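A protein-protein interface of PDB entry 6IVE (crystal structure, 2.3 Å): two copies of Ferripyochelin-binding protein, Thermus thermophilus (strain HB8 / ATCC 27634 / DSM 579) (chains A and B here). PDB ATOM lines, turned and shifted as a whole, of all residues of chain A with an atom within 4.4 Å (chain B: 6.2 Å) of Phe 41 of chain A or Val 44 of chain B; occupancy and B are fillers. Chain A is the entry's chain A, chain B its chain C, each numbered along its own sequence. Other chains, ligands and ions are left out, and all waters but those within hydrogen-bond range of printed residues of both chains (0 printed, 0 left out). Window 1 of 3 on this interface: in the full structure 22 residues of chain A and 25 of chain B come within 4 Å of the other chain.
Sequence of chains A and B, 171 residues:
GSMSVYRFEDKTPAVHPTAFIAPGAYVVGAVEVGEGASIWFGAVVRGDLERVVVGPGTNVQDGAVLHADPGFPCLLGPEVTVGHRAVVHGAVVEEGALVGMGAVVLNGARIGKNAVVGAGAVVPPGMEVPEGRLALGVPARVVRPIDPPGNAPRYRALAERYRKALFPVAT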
ATOM      1  N   ALA A  22     -12.050   5.617  -9.479  1.00  0.00           N
ATOM      2  CA  ALA A  22     -12.289   4.798 -10.655  1.00  0.00           C
ATOM      3  C   ALA A  22     -10.992   4.151 -11.137  1.00  0.00           C
ATOM      4  O   ALA A  22      -9.901   4.685 -10.917  1.00  0.00           O
ATOM      5  CB  ALA A  22     -12.891   5.637 -11.777  1.00  0.00           C
ATOM      6  N   PRO A  23     -11.085   2.989 -11.785  1.00  0.00           N
ATOM      7  CA  PRO A  23      -9.904   2.419 -12.442  1.00  0.00           C
ATOM      8  C   PRO A  23      -9.316   3.393 -13.453  1.00  0.00           C
ATOM      9  O   PRO A  23     -10.036   4.114 -14.145  1.00  0.00           O
ATOM     10  CB  PRO A  23     -10.445   1.152 -13.121  1.00  0.00           C
ATOM     11  CG  PRO A  23     -11.943   1.252 -13.040  1.00  0.00           C
ATOM     12  CD  PRO A  23     -12.238   2.078 -11.836  1.00  0.00           C
ATOM     13  N   TRP A  40     -12.708  10.060 -11.201  1.00  0.00           N
ATOM     14  CA  TRP A  40     -13.196   9.225 -12.286  1.00  0.00           C
ATOM     15  C   TRP A  40     -12.065   8.803 -13.221  1.00  0.00           C
ATOM     16  O   TRP A  40     -10.896   9.149 -13.031  1.00  0.00           O
ATOM     17  CB  TRP A  40     -14.325   9.953 -13.019  1.00  0.00           C
ATOM     18  CG  TRP A  40     -15.523  10.079 -12.136  1.00  0.00           C
ATOM     19  CD1 TRP A  40     -15.753  11.040 -11.193  1.00  0.00           C
ATOM     20  CD2 TRP A  40     -16.636   9.179 -12.070  1.00  0.00           C
ATOM     21  NE1 TRP A  40     -16.950  10.805 -10.560  1.00  0.00           N
ATOM     22  CE2 TRP A  40     -17.511   9.667 -11.079  1.00  0.00           C
ATOM     23  CE3 TRP A  40     -16.982   8.013 -12.760  1.00  0.00           C
ATOM     24  CZ2 TRP A  40     -18.706   9.029 -10.761  1.00  0.00           C
ATOM     25  CZ3 TRP A  40     -18.169   7.383 -12.443  1.00  0.00           C
ATOM     26  CH2 TRP A  40     -19.016   7.892 -11.455  1.00  0.00           C
ATOM     27  N   PHE A  41     -12.437   8.029 -14.244  1.00  0.00           N
ATOM     28  CA  PHE A  41     -11.471   7.325 -15.080  1.00  0.00           C
ATOM     29  C   PHE A  41     -10.482   8.289 -15.719  1.00  0.00           C
ATOM     30  O   PHE A  41     -10.873   9.292 -16.321  1.00  0.00           O
ATOM     31  CB  PHE A  41     -12.197   6.535 -16.173  1.00  0.00           C
ATOM     32  CG  PHE A  41     -13.242   5.587 -15.655  1.00  0.00           C
ATOM     33  CD1 PHE A  41     -14.535   6.027 -15.406  1.00  0.00           C
ATOM     34  CD2 PHE A  41     -12.942   4.251 -15.441  1.00  0.00           C
ATOM     35  CE1 PHE A  41     -15.506   5.155 -14.936  1.00  0.00           C
ATOM     36  CE2 PHE A  41     -13.908   3.374 -14.974  1.00  0.00           C
ATOM     37  CZ  PHE A  41     -15.191   3.827 -14.720  1.00  0.00           C
ATOM     38  N   GLY A  42      -9.195   7.975 -15.596  1.00  0.00           N
ATOM     39  CA  GLY A  42      -8.161   8.770 -16.223  1.00  0.00           C
ATOM     40  C   GLY A  42      -7.860  10.095 -15.557  1.00  0.00           C
ATOM     41  O   GLY A  42      -6.995  10.830 -16.050  1.00  0.00           O
ATOM     42  N   ALA A  43      -8.543  10.433 -14.468  1.00  0.00           N
ATOM     43  CA  ALA A  43      -8.211  11.643 -13.732  1.00  0.00           C
ATOM     44  C   ALA A  43      -6.906  11.454 -12.967  1.00  0.00           C
ATOM     45  O   ALA A  43      -6.525  10.338 -12.606  1.00  0.00           O
ATOM     46  CB  ALA A  43      -9.336  12.014 -12.768  1.00  0.00           C
ATOM     47  N   ASP A  62     -13.696  12.518 -15.566  1.00  0.00           N
ATOM     48  CA  ASP A  62     -12.725  11.775 -16.359  1.00  0.00           C
ATOM     49  C   ASP A  62     -11.717  12.706 -17.019  1.00  0.00           C
ATOM     50  O   ASP A  62     -12.084  13.731 -17.601  1.00  0.00           O
ATOM     51  CB  ASP A  62     -13.446  10.947 -17.425  1.00  0.00           C
ATOM     52  CG  ASP A  62     -14.742  10.343 -16.916  1.00  0.00           C
ATOM     53  OD1 ASP A  62     -15.710  11.107 -16.718  1.00  0.00           O
ATOM     54  OD2 ASP A  62     -14.797   9.109 -16.720  1.00  0.00           O
ATOM     55  N   GLY A  63     -10.439  12.342 -16.926  1.00  0.00           N
ATOM     56  CA  GLY A  63      -9.383  13.087 -17.575  1.00  0.00           C
ATOM     57  C   GLY A  63      -9.032  14.411 -16.937  1.00  0.00           C
ATOM     58  O   GLY A  63      -8.186  15.130 -17.480  1.00  0.00           O
ATOM     59  N   TYR A 162     -21.647   3.207  -8.900  1.00  0.00           N
ATOM     60  CA  TYR A 162     -20.409   2.633  -9.418  1.00  0.00           C
ATOM     61  C   TYR A 162     -19.685   1.823  -8.350  1.00  0.00           C
ATOM     62  O   TYR A 162     -19.069   0.796  -8.654  1.00  0.00           O
ATOM     63  CB  TYR A 162     -19.501   3.733  -9.963  1.00  0.00           C
ATOM     64  CG  TYR A 162     -19.664   3.975 -11.445  1.00  0.00           C
ATOM     65  CD1 TYR A 162     -20.602   4.880 -11.922  1.00  0.00           C
ATOM     66  CD2 TYR A 162     -18.878   3.297 -12.369  1.00  0.00           C
ATOM     67  CE1 TYR A 162     -20.755   5.103 -13.278  1.00  0.00           C
ATOM     68  CE2 TYR A 162     -19.023   3.515 -13.726  1.00  0.00           C
ATOM     69  CZ  TYR A 162     -19.964   4.420 -14.174  1.00  0.00           C
ATOM     70  OH  TYR A 162     -20.115   4.640 -15.525  1.00  0.00           O
ATOM     71  N   LEU A 166     -19.473  -2.130 -10.568  1.00  0.00           N
ATOM     72  CA  LEU A 166     -18.477  -1.891 -11.607  1.00  0.00           C
ATOM     73  C   LEU A 166     -17.605  -3.132 -11.718  1.00  0.00           C
ATOM     74  O   LEU A 166     -16.933  -3.508 -10.752  1.00  0.00           O
ATOM     75  CB  LEU A 166     -17.624  -0.657 -11.300  1.00  0.00           C
ATOM     76  CG  LEU A 166     -16.585  -0.298 -12.366  1.00  0.00           C
ATOM     77  CD1 LEU A 166     -17.256  -0.017 -13.703  1.00  0.00           C
ATOM     78  CD2 LEU A 166     -15.751   0.894 -11.929  1.00  0.00           C
ATOM     79  N   TYR B   6     -15.564  -2.195 -19.148  1.00  0.00           N
ATOM     80  CA  TYR B   6     -16.166  -2.065 -17.826  1.00  0.00           C
ATOM     81  C   TYR B   6     -17.687  -2.093 -17.884  1.00  0.00           C
ATOM     82  O   TYR B   6     -18.315  -1.292 -18.588  1.00  0.00           O
ATOM     83  CB  TYR B   6     -15.663  -0.799 -17.134  1.00  0.00           C
ATOM     84  CG  TYR B   6     -14.192  -0.910 -16.812  1.00  0.00           C
ATOM     85  CD1 TYR B   6     -13.232  -0.520 -17.734  1.00  0.00           C
ATOM     86  CD2 TYR B   6     -13.761  -1.454 -15.607  1.00  0.00           C
ATOM     87  CE1 TYR B   6     -11.883  -0.639 -17.459  1.00  0.00           C
ATOM     88  CE2 TYR B   6     -12.410  -1.575 -15.318  1.00  0.00           C
ATOM     89  CZ  TYR B   6     -11.477  -1.165 -16.252  1.00  0.00           C
ATOM     90  OH  TYR B   6     -10.132  -1.277 -15.984  1.00  0.00           O
ATOM     91  N   GLY B  24      -4.964   1.598 -21.742  1.00  0.00           N
ATOM     92  CA  GLY B  24      -5.257   2.850 -21.082  1.00  0.00           C
ATOM     93  C   GLY B  24      -6.570   3.494 -21.457  1.00  0.00           C
ATOM     94  O   GLY B  24      -6.920   4.525 -20.872  1.00  0.00           O
ATOM     95  N   ALA B  25      -7.302   2.938 -22.416  1.00  0.00           N
ATOM     96  CA  ALA B  25      -8.618   3.445 -22.774  1.00  0.00           C
ATOM     97  C   ALA B  25      -9.671   2.801 -21.883  1.00  0.00           C
ATOM     98  O   ALA B  25      -9.569   1.622 -21.534  1.00  0.00           O
ATOM     99  CB  ALA B  25      -8.926   3.166 -24.246  1.00  0.00           C
ATOM    100  N   TYR B  26     -10.686   3.582 -21.515  1.00  0.00           N
ATOM    101  CA  TYR B  26     -11.726   3.118 -20.597  1.00  0.00           C
ATOM    102  C   TYR B  26     -13.095   3.304 -21.243  1.00  0.00           C
ATOM    103  O   TYR B  26     -13.610   4.422 -21.323  1.00  0.00           O
ATOM    104  CB  TYR B  26     -11.621   3.839 -19.258  1.00  0.00           C
ATOM    105  CG  TYR B  26     -10.355   3.455 -18.534  1.00  0.00           C
ATOM    106  CD1 TYR B  26     -10.314   2.327 -17.728  1.00  0.00           C
ATOM    107  CD2 TYR B  26      -9.188   4.187 -18.698  1.00  0.00           C
ATOM    108  CE1 TYR B  26      -9.151   1.953 -17.081  1.00  0.00           C
ATOM    109  CE2 TYR B  26      -8.020   3.820 -18.057  1.00  0.00           C
ATOM    110  CZ  TYR B  26      -8.009   2.702 -17.251  1.00  0.00           C
ATOM    111  OH  TYR B  26      -6.849   2.334 -16.612  1.00  0.00           O
ATOM    112  N   VAL B  27     -13.672   2.199 -21.702  1.00  0.00           N
ATOM    113  CA  VAL B  27     -15.017   2.168 -22.263  1.00  0.00           C
ATOM    114  C   VAL B  27     -15.942   1.597 -21.193  1.00  0.00           C
ATOM    115  O   VAL B  27     -15.780   0.444 -20.777  1.00  0.00           O
ATOM    116  CB  VAL B  27     -15.062   1.332 -23.552  1.00  0.00           C
ATOM    117  CG1 VAL B  27     -16.400   1.481 -24.241  1.00  0.00           C
ATOM    118  CG2 VAL B  27     -13.919   1.738 -24.479  1.00  0.00           C
ATOM    119  N   VAL B  28     -16.902   2.400 -20.734  1.00  0.00           N
ATOM    120  CA  VAL B  28     -17.656   2.101 -19.522  1.00  0.00           C
ATOM    121  C   VAL B  28     -19.151   2.183 -19.808  1.00  0.00           C
ATOM    122  O   VAL B  28     -19.631   3.177 -20.365  1.00  0.00           O
ATOM    123  CB  VAL B  28     -17.284   3.061 -18.374  1.00  0.00           C
ATOM    124  CG1 VAL B  28     -18.008   2.667 -17.097  1.00  0.00           C
ATOM    125  CG2 VAL B  28     -15.770   3.089 -18.159  1.00  0.00           C
ATOM    126  N   ILE B  39     -10.437   3.352 -30.268  1.00  0.00           N
ATOM    127  CA  ILE B  39     -10.445   4.189 -29.073  1.00  0.00           C
ATOM    128  C   ILE B  39      -9.038   4.141 -28.495  1.00  0.00           C
ATOM    129  O   ILE B  39      -8.580   3.085 -28.043  1.00  0.00           O
ATOM    130  CB  ILE B  39     -11.492   3.719 -28.056  1.00  0.00           C
ATOM    131  CG1 ILE B  39     -12.888   3.793 -28.679  1.00  0.00           C
ATOM    132  CG2 ILE B  39     -11.418   4.551 -26.782  1.00  0.00           C
ATOM    133  CD1 ILE B  39     -13.951   3.069 -27.895  1.00  0.00           C
ATOM    134  N   TRP B  40      -8.355   5.280 -28.500  1.00  0.00           N
ATOM    135  CA  TRP B  40      -6.912   5.315 -28.333  1.00  0.00           C
ATOM    136  C   TRP B  40      -6.516   5.595 -26.883  1.00  0.00           C
ATOM    137  O   TRP B  40      -7.356   5.720 -25.988  1.00  0.00           O
ATOM    138  CB  TRP B  40      -6.319   6.333 -29.306  1.00  0.00           C
ATOM    139  CG  TRP B  40      -6.482   5.870 -30.717  1.00  0.00           C
ATOM    140  CD1 TRP B  40      -7.564   6.070 -31.527  1.00  0.00           C
ATOM    141  CD2 TRP B  40      -5.557   5.080 -31.470  1.00  0.00           C
ATOM    142  NE1 TRP B  40      -7.359   5.466 -32.744  1.00  0.00           N
ATOM    143  CE2 TRP B  40      -6.135   4.851 -32.733  1.00  0.00           C
ATOM    144  CE3 TRP B  40      -4.290   4.551 -31.200  1.00  0.00           C
ATOM    145  CZ2 TRP B  40      -5.490   4.119 -33.728  1.00  0.00           C
ATOM    146  CZ3 TRP B  40      -3.649   3.824 -32.187  1.00  0.00           C
ATOM    147  CH2 TRP B  40      -4.250   3.616 -33.436  1.00  0.00           C
ATOM    148  N   GLY B  42      -5.584   6.442 -23.232  1.00  0.00           N
ATOM    149  CA  GLY B  42      -6.078   7.424 -22.290  1.00  0.00           C
ATOM    150  C   GLY B  42      -7.460   7.970 -22.573  1.00  0.00           C
ATOM    151  O   GLY B  42      -7.947   8.799 -21.798  1.00  0.00           O
ATOM    152  N   ALA B  43      -8.108   7.547 -23.656  1.00  0.00           N
ATOM    153  CA  ALA B  43      -9.463   8.002 -23.929  1.00  0.00           C
ATOM    154  C   ALA B  43     -10.447   7.341 -22.971  1.00  0.00           C
ATOM    155  O   ALA B  43     -10.239   6.218 -22.507  1.00  0.00           O
ATOM    156  CB  ALA B  43      -9.853   7.700 -25.377  1.00  0.00           C
ATOM    157  N   VAL B  44     -11.530   8.051 -22.673  1.00  0.00           N
ATOM    158  CA  VAL B  44     -12.586   7.538 -21.808  1.00  0.00           C
ATOM    159  C   VAL B  44     -13.912   7.703 -22.534  1.00  0.00           C
ATOM    160  O   VAL B  44     -14.278   8.819 -22.923  1.00  0.00           O
ATOM    161  CB  VAL B  44     -12.623   8.250 -20.444  1.00  0.00           C
ATOM    162  CG1 VAL B  44     -13.777   7.716 -19.605  1.00  0.00           C
ATOM    163  CG2 VAL B  44     -11.302   8.072 -19.706  1.00  0.00           C
ATOM    164  N   VAL B  45     -14.627   6.597 -22.719  1.00  0.00           N
ATOM    165  CA  VAL B  45     -15.961   6.594 -23.312  1.00  0.00           C
ATOM    166  C   VAL B  45     -16.884   5.990 -22.265  1.00  0.00           C
ATOM    167  O   VAL B  45     -16.901   4.770 -22.065  1.00  0.00           O
ATOM    168  CB  VAL B  45     -16.014   5.810 -24.628  1.00  0.00           C
ATOM    169  CG1 VAL B  45     -17.415   5.865 -25.213  1.00  0.00           C
ATOM    170  CG2 VAL B  45     -14.993   6.356 -25.616  1.00  0.00           C
ATOM    171  N   ARG B  46     -17.647   6.836 -21.580  1.00  0.00           N
ATOM    172  CA  ARG B  46     -18.438   6.413 -20.433  1.00  0.00           C
ATOM    173  C   ARG B  46     -19.903   6.723 -20.689  1.00  0.00           C
ATOM    174  O   ARG B  46     -20.260   7.873 -20.966  1.00  0.00           O
ATOM    175  CB  ARG B  46     -17.959   7.094 -19.149  1.00  0.00           C
ATOM    176  CG  ARG B  46     -18.859   6.841 -17.949  1.00  0.00           C
ATOM    177  CD  ARG B  46     -18.118   7.066 -16.640  1.00  0.00           C
ATOM    178  NE  ARG B  46     -17.746   8.464 -16.430  1.00  0.00           N
ATOM    179  CZ  ARG B  46     -18.542   9.372 -15.873  1.00  0.00           C
ATOM    180  NH1 ARG B  46     -19.762   9.033 -15.479  1.00  0.00           N
ATOM    181  NH2 ARG B  46     -18.124  10.622 -15.713  1.00  0.00           N
ATOM    182  N   VAL B  60     -11.619   7.571 -31.715  1.00  0.00           N
ATOM    183  CA  VAL B  60     -11.647   8.433 -30.540  1.00  0.00           C
ATOM    184  C   VAL B  60     -10.214   8.508 -30.030  1.00  0.00           C
ATOM    185  O   VAL B  60      -9.732   7.591 -29.357  1.00  0.00           O
ATOM    186  CB  VAL B  60     -12.610   7.907 -29.468  1.00  0.00           C
ATOM    187  CG1 VAL B  60     -12.655   8.849 -28.280  1.00  0.00           C
ATOM    188  CG2 VAL B  60     -14.001   7.725 -30.058  1.00  0.00           C
ATOM    189  N   GLY B  63      -6.627  10.605 -25.098  1.00  0.00           N
ATOM    190  CA  GLY B  63      -7.054  11.569 -24.108  1.00  0.00           C
ATOM    191  C   GLY B  63      -8.438  12.146 -24.309  1.00  0.00           C
ATOM    192  O   GLY B  63      -8.863  12.979 -23.497  1.00  0.00           O
ATOM    193  N   ALA B  64      -9.156  11.741 -25.353  1.00  0.00           N
ATOM    194  CA  ALA B  64     -10.499  12.255 -25.569  1.00  0.00           C
ATOM    195  C   ALA B  64     -11.465  11.688 -24.532  1.00  0.00           C
ATOM    196  O   ALA B  64     -11.261  10.598 -23.990  1.00  0.00           O
ATOM    197  CB  ALA B  64     -10.980  11.920 -26.982  1.00  0.00           C
ATOM    198  N   VAL B  65     -12.525  12.445 -24.249  1.00  0.00           N
ATOM    199  CA  VAL B  65     -13.548  12.040 -23.290  1.00  0.00           C
ATOM    200  C   VAL B  65     -14.914  12.095 -23.963  1.00  0.00           C
ATOM    201  O   VAL B  65     -15.298  13.128 -24.523  1.00  0.00           O
ATOM    202  CB  VAL B  65     -13.539  12.926 -22.028  1.00  0.00           C
ATOM    203  CG1 VAL B  65     -14.695  12.552 -21.117  1.00  0.00           C
ATOM    204  CG2 VAL B  65     -12.216  12.789 -21.287  1.00  0.00           C
ATOM    205  N   LEU B  66     -15.647  10.988 -23.903  1.00  0.00           N
ATOM    206  CA  LEU B  66     -17.038  10.937 -24.330  1.00  0.00           C
ATOM    207  C   LEU B  66     -17.920  10.677 -23.116  1.00  0.00           C
ATOM    208  O   LEU B  66     -17.622   9.793 -22.306  1.00  0.00           O
ATOM    209  CB  LEU B  66     -17.264   9.845 -25.380  1.00  0.00           C
ATOM    210  CG  LEU B  66     -16.545   9.973 -26.723  1.00  0.00           C
ATOM    211  CD1 LEU B  66     -17.129   8.984 -27.721  1.00  0.00           C
ATOM    212  CD2 LEU B  66     -16.632  11.387 -27.254  1.00  0.00           C
ATOM    213  N   HIS B  67     -18.993  11.450 -22.990  1.00  0.00           N
ATOM    214  CA  HIS B  67     -19.985  11.222 -21.951  1.00  0.00           C
ATOM    215  C   HIS B  67     -21.313  11.783 -22.439  1.00  0.00           C
ATOM    216  O   HIS B  67     -21.372  12.535 -23.415  1.00  0.00           O
ATOM    217  CB  HIS B  67     -19.565  11.856 -20.619  1.00  0.00           C
ATOM    218  CG  HIS B  67     -20.403  11.424 -19.454  1.00  0.00           C
ATOM    219  ND1 HIS B  67     -20.761  12.282 -18.436  1.00  0.00           N
ATOM    220  CD2 HIS B  67     -20.950  10.225 -19.145  1.00  0.00           C
ATOM    221  CE1 HIS B  67     -21.495  11.629 -17.552  1.00  0.00           C
ATOM    222  NE2 HIS B  67     -21.626  10.380 -17.960  1.00  0.00           N
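Positions printed for both chains: 40, 42, 43 and 63.
The side-chain carboxylate (OD1) of Asp 62 of chain A lies within salt-bridge range of the guanidinium group (NH2) of Arg 46 of chain B (2.7 Å).
The backbone carbonyl oxygen of Tyr 26 of chain B lies within hydrogen-bond range of the backbone NH of Val 45 of chain B (2.8 Å). N of Tyr 26 of chain B sits at hydrogen-bond distance from O of Ala 43 of chain B, 2.9 Å away. O of Val 44 of chain B sits at hydrogen-bond distance from N of Leu 66 of chain B (2.7 Å). N of Arg 46 of chain B is in hydrogen-bond range of O of Leu 66 of chain B (3.0 Å). The backbone NH (N) of Val 44 of chain B lies within hydrogen-bond range of the backbone carbonyl oxygen (O) of Ala 64 of chain B, at 2.9 Å. The backbone NH of Gly 63 of chain A lies within hydrogen-bond range of the backbone carbonyl oxygen of Phe 41 of chain A.
Of the 10 printed residues of chain A, 6 touch a printed residue of chain B. Printed residues of chain B that touch a printed residue of chain A: Tyr 6, Tyr 26, Val 28, Val 44, Arg 46 and Val 65. Among the printed residues, 13 pairs touch across the chains.
Among the printed residues, merely in contact across the chains: Pro 23 of chain A with Tyr 6 of chain B, Pro 23 of chain A with Tyr 26 of chain B, Trp 40 of chain A with Arg 46 of chain B, Phe 41 of chain A with Tyr 26 of chain B, Phe 41 of chain A with Val 28 of chain B, Phe 41 of chain A with Val 44 of chain B, Phe 41 of chain A with Arg 46 of chain B, Asp 62 of chain A with Val 44 of chain B, Asp 62 of chain A with Val 65 of chain B, Tyr 162 of chain A with Val 28 of chain B, Tyr 162 of chain A with Arg 46 of chain B and Leu 166 of chain A with Tyr 6 of chain B.
Of the printed residues of chain B, Trp 40 of chain A touches Arg 46 (3.7 Å). Phe 41 of chain A touches just these residues of chain B: Tyr 26, Val 28, Val 44 and Arg 46. Printed residues of chain B within 4 Å of Asp 62 of chain A: Val 44 (3.4 Å), Arg 46 (2.7 Å) and Val 65 (3.8 Å). Printed residues of chain A within 4 Å of Val 28 of chain B: Phe 41 and Tyr 162. Val 44 of chain B touches just these residues of chain A: Phe 41 (3.6 Å) and Asp 62 (3.4 Å). Of the printed residues of chain A, Val 65 of chain B touches Asp 62 (3.8 Å). The nearest residue of chain B that does not touch Phe 41 of chain A is Tyr 6 of chain B (4.7 Å). The nearest printed residue of chain B that does not touch Asp 62 of chain A is His 67 of chain B (5.4 Å).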
